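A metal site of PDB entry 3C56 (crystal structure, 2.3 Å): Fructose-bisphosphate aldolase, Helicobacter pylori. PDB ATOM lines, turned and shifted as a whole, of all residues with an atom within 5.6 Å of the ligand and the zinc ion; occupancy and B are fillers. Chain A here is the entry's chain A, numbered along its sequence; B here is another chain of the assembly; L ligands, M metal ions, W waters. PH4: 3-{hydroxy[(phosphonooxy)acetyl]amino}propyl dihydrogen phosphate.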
ATOM      1  N   ASN A  23      19.622  21.285   4.917  1.00  0.00           N
ATOM      2  CA  ASN A  23      19.837  21.828   6.247  1.00  0.00           C
ATOM      3  C   ASN A  23      19.914  20.736   7.296  1.00  0.00           C
ATOM      4  O   ASN A  23      19.351  19.655   7.138  1.00  0.00           O
ATOM      5  CB  ASN A  23      18.735  22.826   6.609  1.00  0.00           C
ATOM      6  CG  ASN A  23      18.710  24.032   5.695  1.00  0.00           C
ATOM      7  OD1 ASN A  23      18.404  23.913   4.507  1.00  0.00           O
ATOM      8  ND2 ASN A  23      19.028  25.203   6.245  1.00  0.00           N
ATOM      9  N   GLN A  47      24.111  22.985   4.747  1.00  0.00           N
ATOM     10  CA  GLN A  47      23.944  24.339   5.261  1.00  0.00           C
ATOM     11  C   GLN A  47      23.259  24.390   6.617  1.00  0.00           C
ATOM     12  O   GLN A  47      22.507  23.488   6.983  1.00  0.00           O
ATOM     13  CB  GLN A  47      23.177  25.196   4.238  1.00  0.00           C
ATOM     14  CG  GLN A  47      21.846  24.610   3.803  1.00  0.00           C
ATOM     15  CD  GLN A  47      21.202  25.413   2.689  1.00  0.00           C
ATOM     16  OE1 GLN A  47      21.893  26.018   1.877  1.00  0.00           O
ATOM     17  NE2 GLN A  47      19.882  25.411   2.651  1.00  0.00           N
ATOM     18  N   SER A  49      21.213  27.271   9.235  1.00  0.00           N
ATOM     19  CA  SER A  49      20.665  28.589   9.502  1.00  0.00           C
ATOM     20  C   SER A  49      21.295  29.164  10.765  1.00  0.00           C
ATOM     21  O   SER A  49      21.976  28.455  11.512  1.00  0.00           O
ATOM     22  CB  SER A  49      19.148  28.508   9.673  1.00  0.00           C
ATOM     23  OG  SER A  49      18.809  27.655  10.751  1.00  0.00           O
ATOM     24  N   GLY A  51      19.638  30.007  13.244  1.00  0.00           N
ATOM     25  CA  GLY A  51      18.910  29.348  14.315  1.00  0.00           C
ATOM     26  C   GLY A  51      19.501  27.993  14.636  1.00  0.00           C
ATOM     27  O   GLY A  51      19.521  27.575  15.801  1.00  0.00           O
ATOM     28  N   ALA A  52      19.977  27.309  13.607  1.00  0.00           N
ATOM     29  CA  ALA A  52      20.614  26.001  13.785  1.00  0.00           C
ATOM     30  C   ALA A  52      21.962  26.163  14.485  1.00  0.00           C
ATOM     31  O   ALA A  52      22.312  25.371  15.354  1.00  0.00           O
ATOM     32  CB  ALA A  52      20.795  25.322  12.442  1.00  0.00           C
ATOM     33  N   ASP A  82      23.337  29.402   6.084  1.00  0.00           N
ATOM     34  CA  ASP A  82      22.045  29.667   5.478  1.00  0.00           C
ATOM     35  C   ASP A  82      21.370  30.894   6.083  1.00  0.00           C
ATOM     36  O   ASP A  82      21.074  30.935   7.278  1.00  0.00           O
ATOM     37  CB  ASP A  82      21.139  28.442   5.602  1.00  0.00           C
ATOM     38  CG  ASP A  82      19.876  28.576   4.783  1.00  0.00           C
ATOM     39  OD1 ASP A  82      19.835  29.420   3.857  1.00  0.00           O
ATOM     40  OD2 ASP A  82      18.914  27.829   5.068  1.00  0.00           O
ATOM     41  N   HIS A  83      21.132  31.902   5.237  1.00  0.00           N
ATOM     42  CA  HIS A  83      20.443  33.115   5.656  1.00  0.00           C
ATOM     43  C   HIS A  83      21.186  33.887   6.748  1.00  0.00           C
ATOM     44  O   HIS A  83      20.630  34.163   7.810  1.00  0.00           O
ATOM     45  CB  HIS A  83      19.011  32.818   6.103  1.00  0.00           C
ATOM     46  CG  HIS A  83      18.058  32.591   4.969  1.00  0.00           C
ATOM     47  ND1 HIS A  83      17.503  33.622   4.245  1.00  0.00           N
ATOM     48  CD2 HIS A  83      17.562  31.451   4.440  1.00  0.00           C
ATOM     49  CE1 HIS A  83      16.703  33.128   3.315  1.00  0.00           C
ATOM     50  NE2 HIS A  83      16.722  31.810   3.421  1.00  0.00           N
ATOM     51  N   LEU A 138      11.094  36.546  -0.642  1.00  0.00           N
ATOM     52  CA  LEU A 138      10.607  35.166  -0.675  1.00  0.00           C
ATOM     53  C   LEU A 138       9.150  35.081  -0.262  1.00  0.00           C
ATOM     54  O   LEU A 138       8.852  34.750   0.890  1.00  0.00           O
ATOM     55  CB  LEU A 138      11.449  34.278   0.253  1.00  0.00           C
ATOM     56  CG  LEU A 138      12.783  33.811  -0.301  1.00  0.00           C
ATOM     57  CD1 LEU A 138      13.497  32.919   0.709  1.00  0.00           C
ATOM     58  CD2 LEU A 138      12.576  33.115  -1.638  1.00  0.00           C
ATOM     59  N   SER A 179       8.679  29.818  -1.358  1.00  0.00           N
ATOM     60  CA  SER A 179       8.695  30.301   0.019  1.00  0.00           C
ATOM     61  C   SER A 179       8.968  29.144   0.966  1.00  0.00           C
ATOM     62  O   SER A 179       8.767  27.981   0.605  1.00  0.00           O
ATOM     63  CB  SER A 179       7.366  30.974   0.365  1.00  0.00           C
ATOM     64  OG  SER A 179       6.301  30.046   0.341  1.00  0.00           O
ATOM     65  N   HIS A 180       9.422  29.444   2.175  1.00  0.00           N
ATOM     66  CA  HIS A 180       9.724  28.418   3.157  1.00  0.00           C
ATOM     67  C   HIS A 180       8.452  27.888   3.816  1.00  0.00           C
ATOM     68  O   HIS A 180       7.423  28.570   3.846  1.00  0.00           O
ATOM     69  CB  HIS A 180      10.673  28.954   4.238  1.00  0.00           C
ATOM     70  CG  HIS A 180      11.853  29.707   3.678  1.00  0.00           C
ATOM     71  ND1 HIS A 180      12.249  30.927   4.180  1.00  0.00           N
ATOM     72  CD2 HIS A 180      12.704  29.410   2.673  1.00  0.00           C
ATOM     73  CE1 HIS A 180      13.306  31.352   3.496  1.00  0.00           C
ATOM     74  NE2 HIS A 180      13.591  30.454   2.572  1.00  0.00           N
ATOM     75  N   GLY A 181       8.525  26.676   4.342  1.00  0.00           N
ATOM     76  CA  GLY A 181       7.390  26.062   5.023  1.00  0.00           C
ATOM     77  C   GLY A 181       6.695  25.020   4.173  1.00  0.00           C
ATOM     78  O   GLY A 181       7.023  24.833   2.997  1.00  0.00           O
ATOM     79  N   ALA A 182       5.733  24.326   4.765  1.00  0.00           N
ATOM     80  CA  ALA A 182       4.990  23.291   4.057  1.00  0.00           C
ATOM     81  C   ALA A 182       3.821  23.869   3.269  1.00  0.00           C
ATOM     82  O   ALA A 182       3.176  23.168   2.489  1.00  0.00           O
ATOM     83  CB  ALA A 182       4.514  22.219   5.021  1.00  0.00           C
ATOM     84  N   LYS A 184       3.297  26.456   0.661  1.00  0.00           N
ATOM     85  CA  LYS A 184       3.838  27.372  -0.329  1.00  0.00           C
ATOM     86  C   LYS A 184       2.768  27.854  -1.302  1.00  0.00           C
ATOM     87  O   LYS A 184       2.718  29.031  -1.647  1.00  0.00           O
ATOM     88  CB  LYS A 184       4.960  26.699  -1.114  1.00  0.00           C
ATOM     89  CG  LYS A 184       5.995  26.000  -0.246  1.00  0.00           C
ATOM     90  CD  LYS A 184       7.025  25.279  -1.091  1.00  0.00           C
ATOM     91  CE  LYS A 184       7.966  24.470  -0.230  1.00  0.00           C
ATOM     92  NZ  LYS A 184       8.586  25.292   0.837  1.00  0.00           N
ATOM     93  N   LEU A 209      17.655  28.258  -5.480  1.00  0.00           N
ATOM     94  CA  LEU A 209      16.214  28.262  -5.260  1.00  0.00           C
ATOM     95  C   LEU A 209      15.895  27.975  -3.793  1.00  0.00           C
ATOM     96  O   LEU A 209      16.222  26.900  -3.275  1.00  0.00           O
ATOM     97  CB  LEU A 209      15.520  27.229  -6.151  1.00  0.00           C
ATOM     98  CG  LEU A 209      13.991  27.314  -6.206  1.00  0.00           C
ATOM     99  CD1 LEU A 209      13.557  28.552  -6.972  1.00  0.00           C
ATOM    100  CD2 LEU A 209      13.395  26.062  -6.845  1.00  0.00           C
ATOM    101  N   HIS A 210      15.260  28.932  -3.132  1.00  0.00           N
ATOM    102  CA  HIS A 210      14.884  28.780  -1.734  1.00  0.00           C
ATOM    103  C   HIS A 210      13.485  28.188  -1.617  1.00  0.00           C
ATOM    104  O   HIS A 210      12.716  28.200  -2.579  1.00  0.00           O
ATOM    105  CB  HIS A 210      14.942  30.125  -1.001  1.00  0.00           C
ATOM    106  CG  HIS A 210      16.335  30.526  -0.605  1.00  0.00           C
ATOM    107  ND1 HIS A 210      16.720  30.652   0.706  1.00  0.00           N
ATOM    108  CD2 HIS A 210      17.421  30.837  -1.354  1.00  0.00           C
ATOM    109  CE1 HIS A 210      17.988  31.023   0.755  1.00  0.00           C
ATOM    110  NE2 HIS A 210      18.434  31.148  -0.479  1.00  0.00           N
ATOM    111  N   GLY A 211      13.156  27.666  -0.446  1.00  0.00           N
ATOM    112  CA  GLY A 211      11.855  27.060  -0.210  1.00  0.00           C
ATOM    113  C   GLY A 211      11.482  26.101  -1.321  1.00  0.00           C
ATOM    114  O   GLY A 211      10.424  26.241  -1.940  1.00  0.00           O
ATOM    115  N   ALA A 212      12.352  25.129  -1.583  1.00  0.00           N
ATOM    116  CA  ALA A 212      12.167  24.233  -2.716  1.00  0.00           C
ATOM    117  C   ALA A 212      11.787  22.813  -2.305  1.00  0.00           C
ATOM    118  O   ALA A 212      12.018  21.862  -3.050  1.00  0.00           O
ATOM    119  CB  ALA A 212      13.421  24.220  -3.576  1.00  0.00           C
ATOM    120  N   SER A 213      11.224  22.670  -1.109  1.00  0.00           N
ATOM    121  CA  SER A 213      10.728  21.378  -0.661  1.00  0.00           C
ATOM    122  C   SER A 213       9.495  20.977  -1.471  1.00  0.00           C
ATOM    123  O   SER A 213       8.687  21.832  -1.833  1.00  0.00           O
ATOM    124  CB  SER A 213      10.383  21.414   0.828  1.00  0.00           C
ATOM    125  OG  SER A 213      11.532  21.186   1.621  1.00  0.00           O
ATOM    126  N   ASN A 253      17.610  24.531  -2.070  1.00  0.00           N
ATOM    127  CA  ASN A 253      17.432  24.473  -0.623  1.00  0.00           C
ATOM    128  C   ASN A 253      16.312  23.516  -0.203  1.00  0.00           C
ATOM    129  O   ASN A 253      15.153  23.692  -0.584  1.00  0.00           O
ATOM    130  CB  ASN A 253      17.174  25.871  -0.064  1.00  0.00           C
ATOM    131  CG  ASN A 253      18.405  26.767  -0.153  1.00  0.00           C
ATOM    132  OD1 ASN A 253      19.323  26.501  -0.926  1.00  0.00           O
ATOM    133  ND2 ASN A 253      18.418  27.835   0.637  1.00  0.00           N
ATOM    134  N   THR A 254      16.679  22.510   0.578  1.00  0.00           N
ATOM    135  CA  THR A 254      15.720  21.533   1.085  1.00  0.00           C
ATOM    136  C   THR A 254      15.826  21.399   2.591  1.00  0.00           C
ATOM    137  O   THR A 254      16.910  21.155   3.135  1.00  0.00           O
ATOM    138  CB  THR A 254      15.929  20.146   0.445  1.00  0.00           C
ATOM    139  OG1 THR A 254      16.167  20.294  -0.962  1.00  0.00           O
ATOM    140  CG2 THR A 254      14.717  19.271   0.667  1.00  0.00           C
ATOM    141  N   ASP A 255      14.697  21.553   3.286  1.00  0.00           N
ATOM    142  CA  ASP A 255      14.675  21.516   4.742  1.00  0.00           C
ATOM    143  C   ASP A 255      13.383  20.907   5.276  1.00  0.00           C
ATOM    144  O   ASP A 255      13.418  19.956   6.048  1.00  0.00           O
ATOM    145  CB  ASP A 255      14.867  22.924   5.309  1.00  0.00           C
ATOM    146  CG  ASP A 255      15.133  22.929   6.810  1.00  0.00           C
ATOM    147  OD1 ASP A 255      14.697  21.993   7.498  1.00  0.00           O
ATOM    148  OD2 ASP A 255      15.777  23.885   7.292  1.00  0.00           O
ATOM    149  N   THR A 256      12.251  21.456   4.848  1.00  0.00           N
ATOM    150  CA  THR A 256      10.949  21.002   5.324  1.00  0.00           C
ATOM    151  C   THR A 256      10.743  19.508   5.086  1.00  0.00           C
ATOM    152  O   THR A 256      10.288  18.789   5.980  1.00  0.00           O
ATOM    153  CB  THR A 256       9.799  21.780   4.660  1.00  0.00           C
ATOM    154  OG1 THR A 256       9.884  23.163   5.029  1.00  0.00           O
ATOM    155  CG2 THR A 256       8.457  21.227   5.122  1.00  0.00           C
ATOM    156  N   ASP A 257      11.065  19.046   3.891  1.00  0.00           N
ATOM    157  CA  ASP A 257      10.940  17.631   3.554  1.00  0.00           C
ATOM    158  C   ASP A 257      11.673  16.748   4.555  1.00  0.00           C
ATOM    159  O   ASP A 257      11.166  15.708   4.971  1.00  0.00           O
ATOM    160  CB  ASP A 257      11.463  17.368   2.134  1.00  0.00           C
ATOM    161  CG  ASP A 257      10.533  17.887   1.057  1.00  0.00           C
ATOM    162  OD1 ASP A 257       9.361  18.162   1.376  1.00  0.00           O
ATOM    163  OD2 ASP A 257      10.977  18.032  -0.093  1.00  0.00           O
ATOM    164  N   ARG A 259      12.608  17.551   7.757  1.00  0.00           N
ATOM    165  CA  ARG A 259      11.936  17.644   9.050  1.00  0.00           C
ATOM    166  C   ARG A 259      10.733  16.710   9.126  1.00  0.00           C
ATOM    167  O   ARG A 259      10.629  15.871  10.014  1.00  0.00           O
ATOM    168  CB  ARG A 259      11.483  19.079   9.329  1.00  0.00           C
ATOM    169  CG  ARG A 259      12.601  20.115   9.371  1.00  0.00           C
ATOM    170  CD  ARG A 259      12.073  21.466   9.848  1.00  0.00           C
ATOM    171  NE  ARG A 259      13.059  22.530   9.689  1.00  0.00           N
ATOM    172  CZ  ARG A 259      12.849  23.790  10.062  1.00  0.00           C
ATOM    173  NH1 ARG A 259      11.690  24.144  10.612  1.00  0.00           N
ATOM    174  NH2 ARG A 259      13.791  24.697   9.880  1.00  0.00           N
ATOM    175  N   ASP B 278       9.469  20.754  13.678  1.00  0.00           N
ATOM    176  CA  ASP B 278      10.761  21.389  13.883  1.00  0.00           C
ATOM    177  C   ASP B 278      11.499  20.666  15.007  1.00  0.00           C
ATOM    178  O   ASP B 278      11.126  20.787  16.179  1.00  0.00           O
ATOM    179  CB  ASP B 278      10.590  22.868  14.220  1.00  0.00           C
ATOM    180  CG  ASP B 278      11.919  23.597  14.351  1.00  0.00           C
ATOM    181  OD1 ASP B 278      12.970  22.937  14.360  1.00  0.00           O
ATOM    182  OD2 ASP B 278      11.902  24.850  14.445  1.00  0.00           O
ATOM    183  N   ARG B 280      14.112  21.125  16.657  1.00  0.00           N
ATOM    184  CA  ARG B 280      14.580  21.969  17.758  1.00  0.00           C
ATOM    185  C   ARG B 280      13.466  22.244  18.776  1.00  0.00           C
ATOM    186  O   ARG B 280      13.748  22.506  19.948  1.00  0.00           O
ATOM    187  CB  ARG B 280      15.156  23.273  17.212  1.00  0.00           C
ATOM    188  CG  ARG B 280      16.455  23.100  16.451  1.00  0.00           C
ATOM    189  CD  ARG B 280      16.809  24.338  15.650  1.00  0.00           C
ATOM    190  NE  ARG B 280      15.779  24.656  14.672  1.00  0.00           N
ATOM    191  CZ  ARG B 280      15.924  25.566  13.707  1.00  0.00           C
ATOM    192  NH1 ARG B 280      17.052  26.250  13.606  1.00  0.00           N
ATOM    193  NH2 ARG B 280      14.941  25.798  12.850  1.00  0.00           N
HETATM  194  N3  PH4 L   1      16.161  27.341   3.821  1.00  0.00           N
HETATM  195  C4  PH4 L   1      16.116  26.873   5.207  1.00  0.00           C
HETATM  196  C5  PH4 L   1      16.125  28.095   6.155  1.00  0.00           C
HETATM  197  C6  PH4 L   1      16.215  27.616   7.615  1.00  0.00           C
HETATM  198  O62 PH4 L   1      16.316  26.927  10.444  1.00  0.00           O
HETATM  199  P6  PH4 L   1      15.185  28.044  10.017  1.00  0.00           P
HETATM  200  O63 PH4 L   1      13.699  27.526  10.485  1.00  0.00           O
HETATM  201  O61 PH4 L   1      15.493  29.313  10.651  1.00  0.00           O
HETATM  202  O6  PH4 L   1      15.209  28.234   8.368  1.00  0.00           O
HETATM  203  O3  PH4 L   1      17.223  28.139   3.380  1.00  0.00           O
HETATM  204  C2  PH4 L   1      15.099  26.951   2.894  1.00  0.00           C
HETATM  205  O2  PH4 L   1      15.129  27.328   1.766  1.00  0.00           O
HETATM  206  C1  PH4 L   1      13.928  26.070   3.374  1.00  0.00           C
HETATM  207  O1  PH4 L   1      13.158  25.674   2.272  1.00  0.00           O
HETATM  208  P1  PH4 L   1      11.872  24.667   2.500  1.00  0.00           P
HETATM  209  O12 PH4 L   1      10.984  25.179   3.790  1.00  0.00           O
HETATM  210  O13 PH4 L   1      12.422  23.140   2.785  1.00  0.00           O
HETATM  211  O11 PH4 L   1      11.033  24.664   1.302  1.00  0.00           O
HETATM  212 ZN    ZN M   1      15.787  30.021   2.567  1.00  0.00          ZN
HETATM  213  O   HOH W   1      15.326  29.185  13.290  1.00  0.00           O
HETATM  214  O   HOH W   2      12.386  25.578   6.236  1.00  0.00           O
HETATM  215  O   HOH W   3      17.518  30.813  11.086  1.00  0.00           O
HETATM  216  O   HOH W   4      17.255  30.750   8.237  1.00  0.00           O
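Water W3 lies within hydrogen-bond range of an oxygen (O61) of the ligand, the backbone NH of Gly 51 and the side-chain hydroxyl of Ser 49. Water W1 lies within hydrogen-bond range of an oxygen (O61) of the ligand and the guanidinium group of Arg 280 of chain B.
The guanidinium group (NH2) of Arg 259 is in salt-bridge range of an oxygen (O63) of the ligand (2.9 Å). OG of Ser 213 sits at hydrogen-bond distance from O13 of the ligand (2.4 Å). An oxygen (O13) of the ligand sits at hydrogen-bond distance from the backbone NH (N) of Thr 256. The backbone NH (N) of Gly 211 sits at hydrogen-bond distance from an oxygen (O2) of the ligand (3.0 Å). The side-chain hydroxyl (OG) of Ser 49 sits at hydrogen-bond distance from an oxygen (O62) of the ligand, at 2.6 Å. NH2 of Arg 280 of chain B is in salt-bridge range of O62 of the ligand, 3.0 Å away. The backbone NH (N) of Gly 181 lies within hydrogen-bond range of an oxygen (O12) of the ligand, 2.9 Å away. NZ of Lys 184 is in salt-bridge range of O11 of the ligand (2.6 Å). O3 of the ligand sits close to ND2 of Asn 253, at 3.0 Å. The backbone NH (N) of Ser 213 lies within hydrogen-bond range of an oxygen (O11) of the ligand (3.1 Å). The backbone NH of Asp 255 is in hydrogen-bond range of an oxygen (O13) of the ligand (2.8 Å). The side-chain hydroxyl (OG1) of Thr 256 is in hydrogen-bond range of an oxygen (O12) of the ligand. OD2 of Asp 82 lies close to O3 of the ligand. The backbone NH of Ala 212 lies within hydrogen-bond range of an oxygen (O11) of the ligand, 3.2 Å away.
Asn 23 touches the ligand (ND2 to C4, 3.5 Å). Gln 47 touches the ligand (NE2 to O3, 3.9 Å). Thr 254 touches the ligand (C to O13, 3.8 Å). Hydrophobic or aromatic side chains that line the ligand: His 83, His 180 and His 210. Within 4 Å of the ligand: Asn 23, Gln 47, Ser 49, Asp 82, His 83, His 180, Gly 181, Lys 184, His 210, Gly 211, Ala 212, Ser 213, Asn 253, Thr 254, Asp 255, Thr 256, Arg 259 and Arg 280 of chain B.
Merely in contact with the zinc ion: Asn 253 (3.9 Å). Within 4 Å of the zinc ion: His 83, His 180, His 210 and Asn 253. The nearest printed residue that does not touch the zinc ion is Leu 138 (4.1 Å).
The zinc ion is bound by a ring nitrogen (ND1) of His 210 (2.2 Å), a ring nitrogen (NE2) of His 83 (2.2 Å), a ring nitrogen (NE2) of His 180 (2.2 Å) and an oxygen (O3) of the ligand (2.5 Å).
The backbone carbonyl oxygen (O) of Asn 253 sits at hydrogen-bond distance from the backbone NH (N) of Ala 212 (3.3 Å). OD2 of Asp 278 of chain B is in salt-bridge range of NH1 of Arg 259, 3.9 Å away. N of Asp 257 sits at hydrogen-bond distance from OG of Ser 213. The backbone NH of Asn 23 is in hydrogen-bond range of the backbone carbonyl oxygen of Thr 254. The side-chain amide nitrogen of Asn 23 sits at hydrogen-bond distance from the side-chain carboxylate of Asp 82 (2.9 Å). NZ of Lys 184 sits at hydrogen-bond distance from O of Gly 181 (2.7 Å). N of Thr 256 sits at hydrogen-bond distance from OG of Ser 213, 3.3 Å away. NZ of Lys 184 lies within hydrogen-bond range of O of Ser 179 (2.7 Å).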
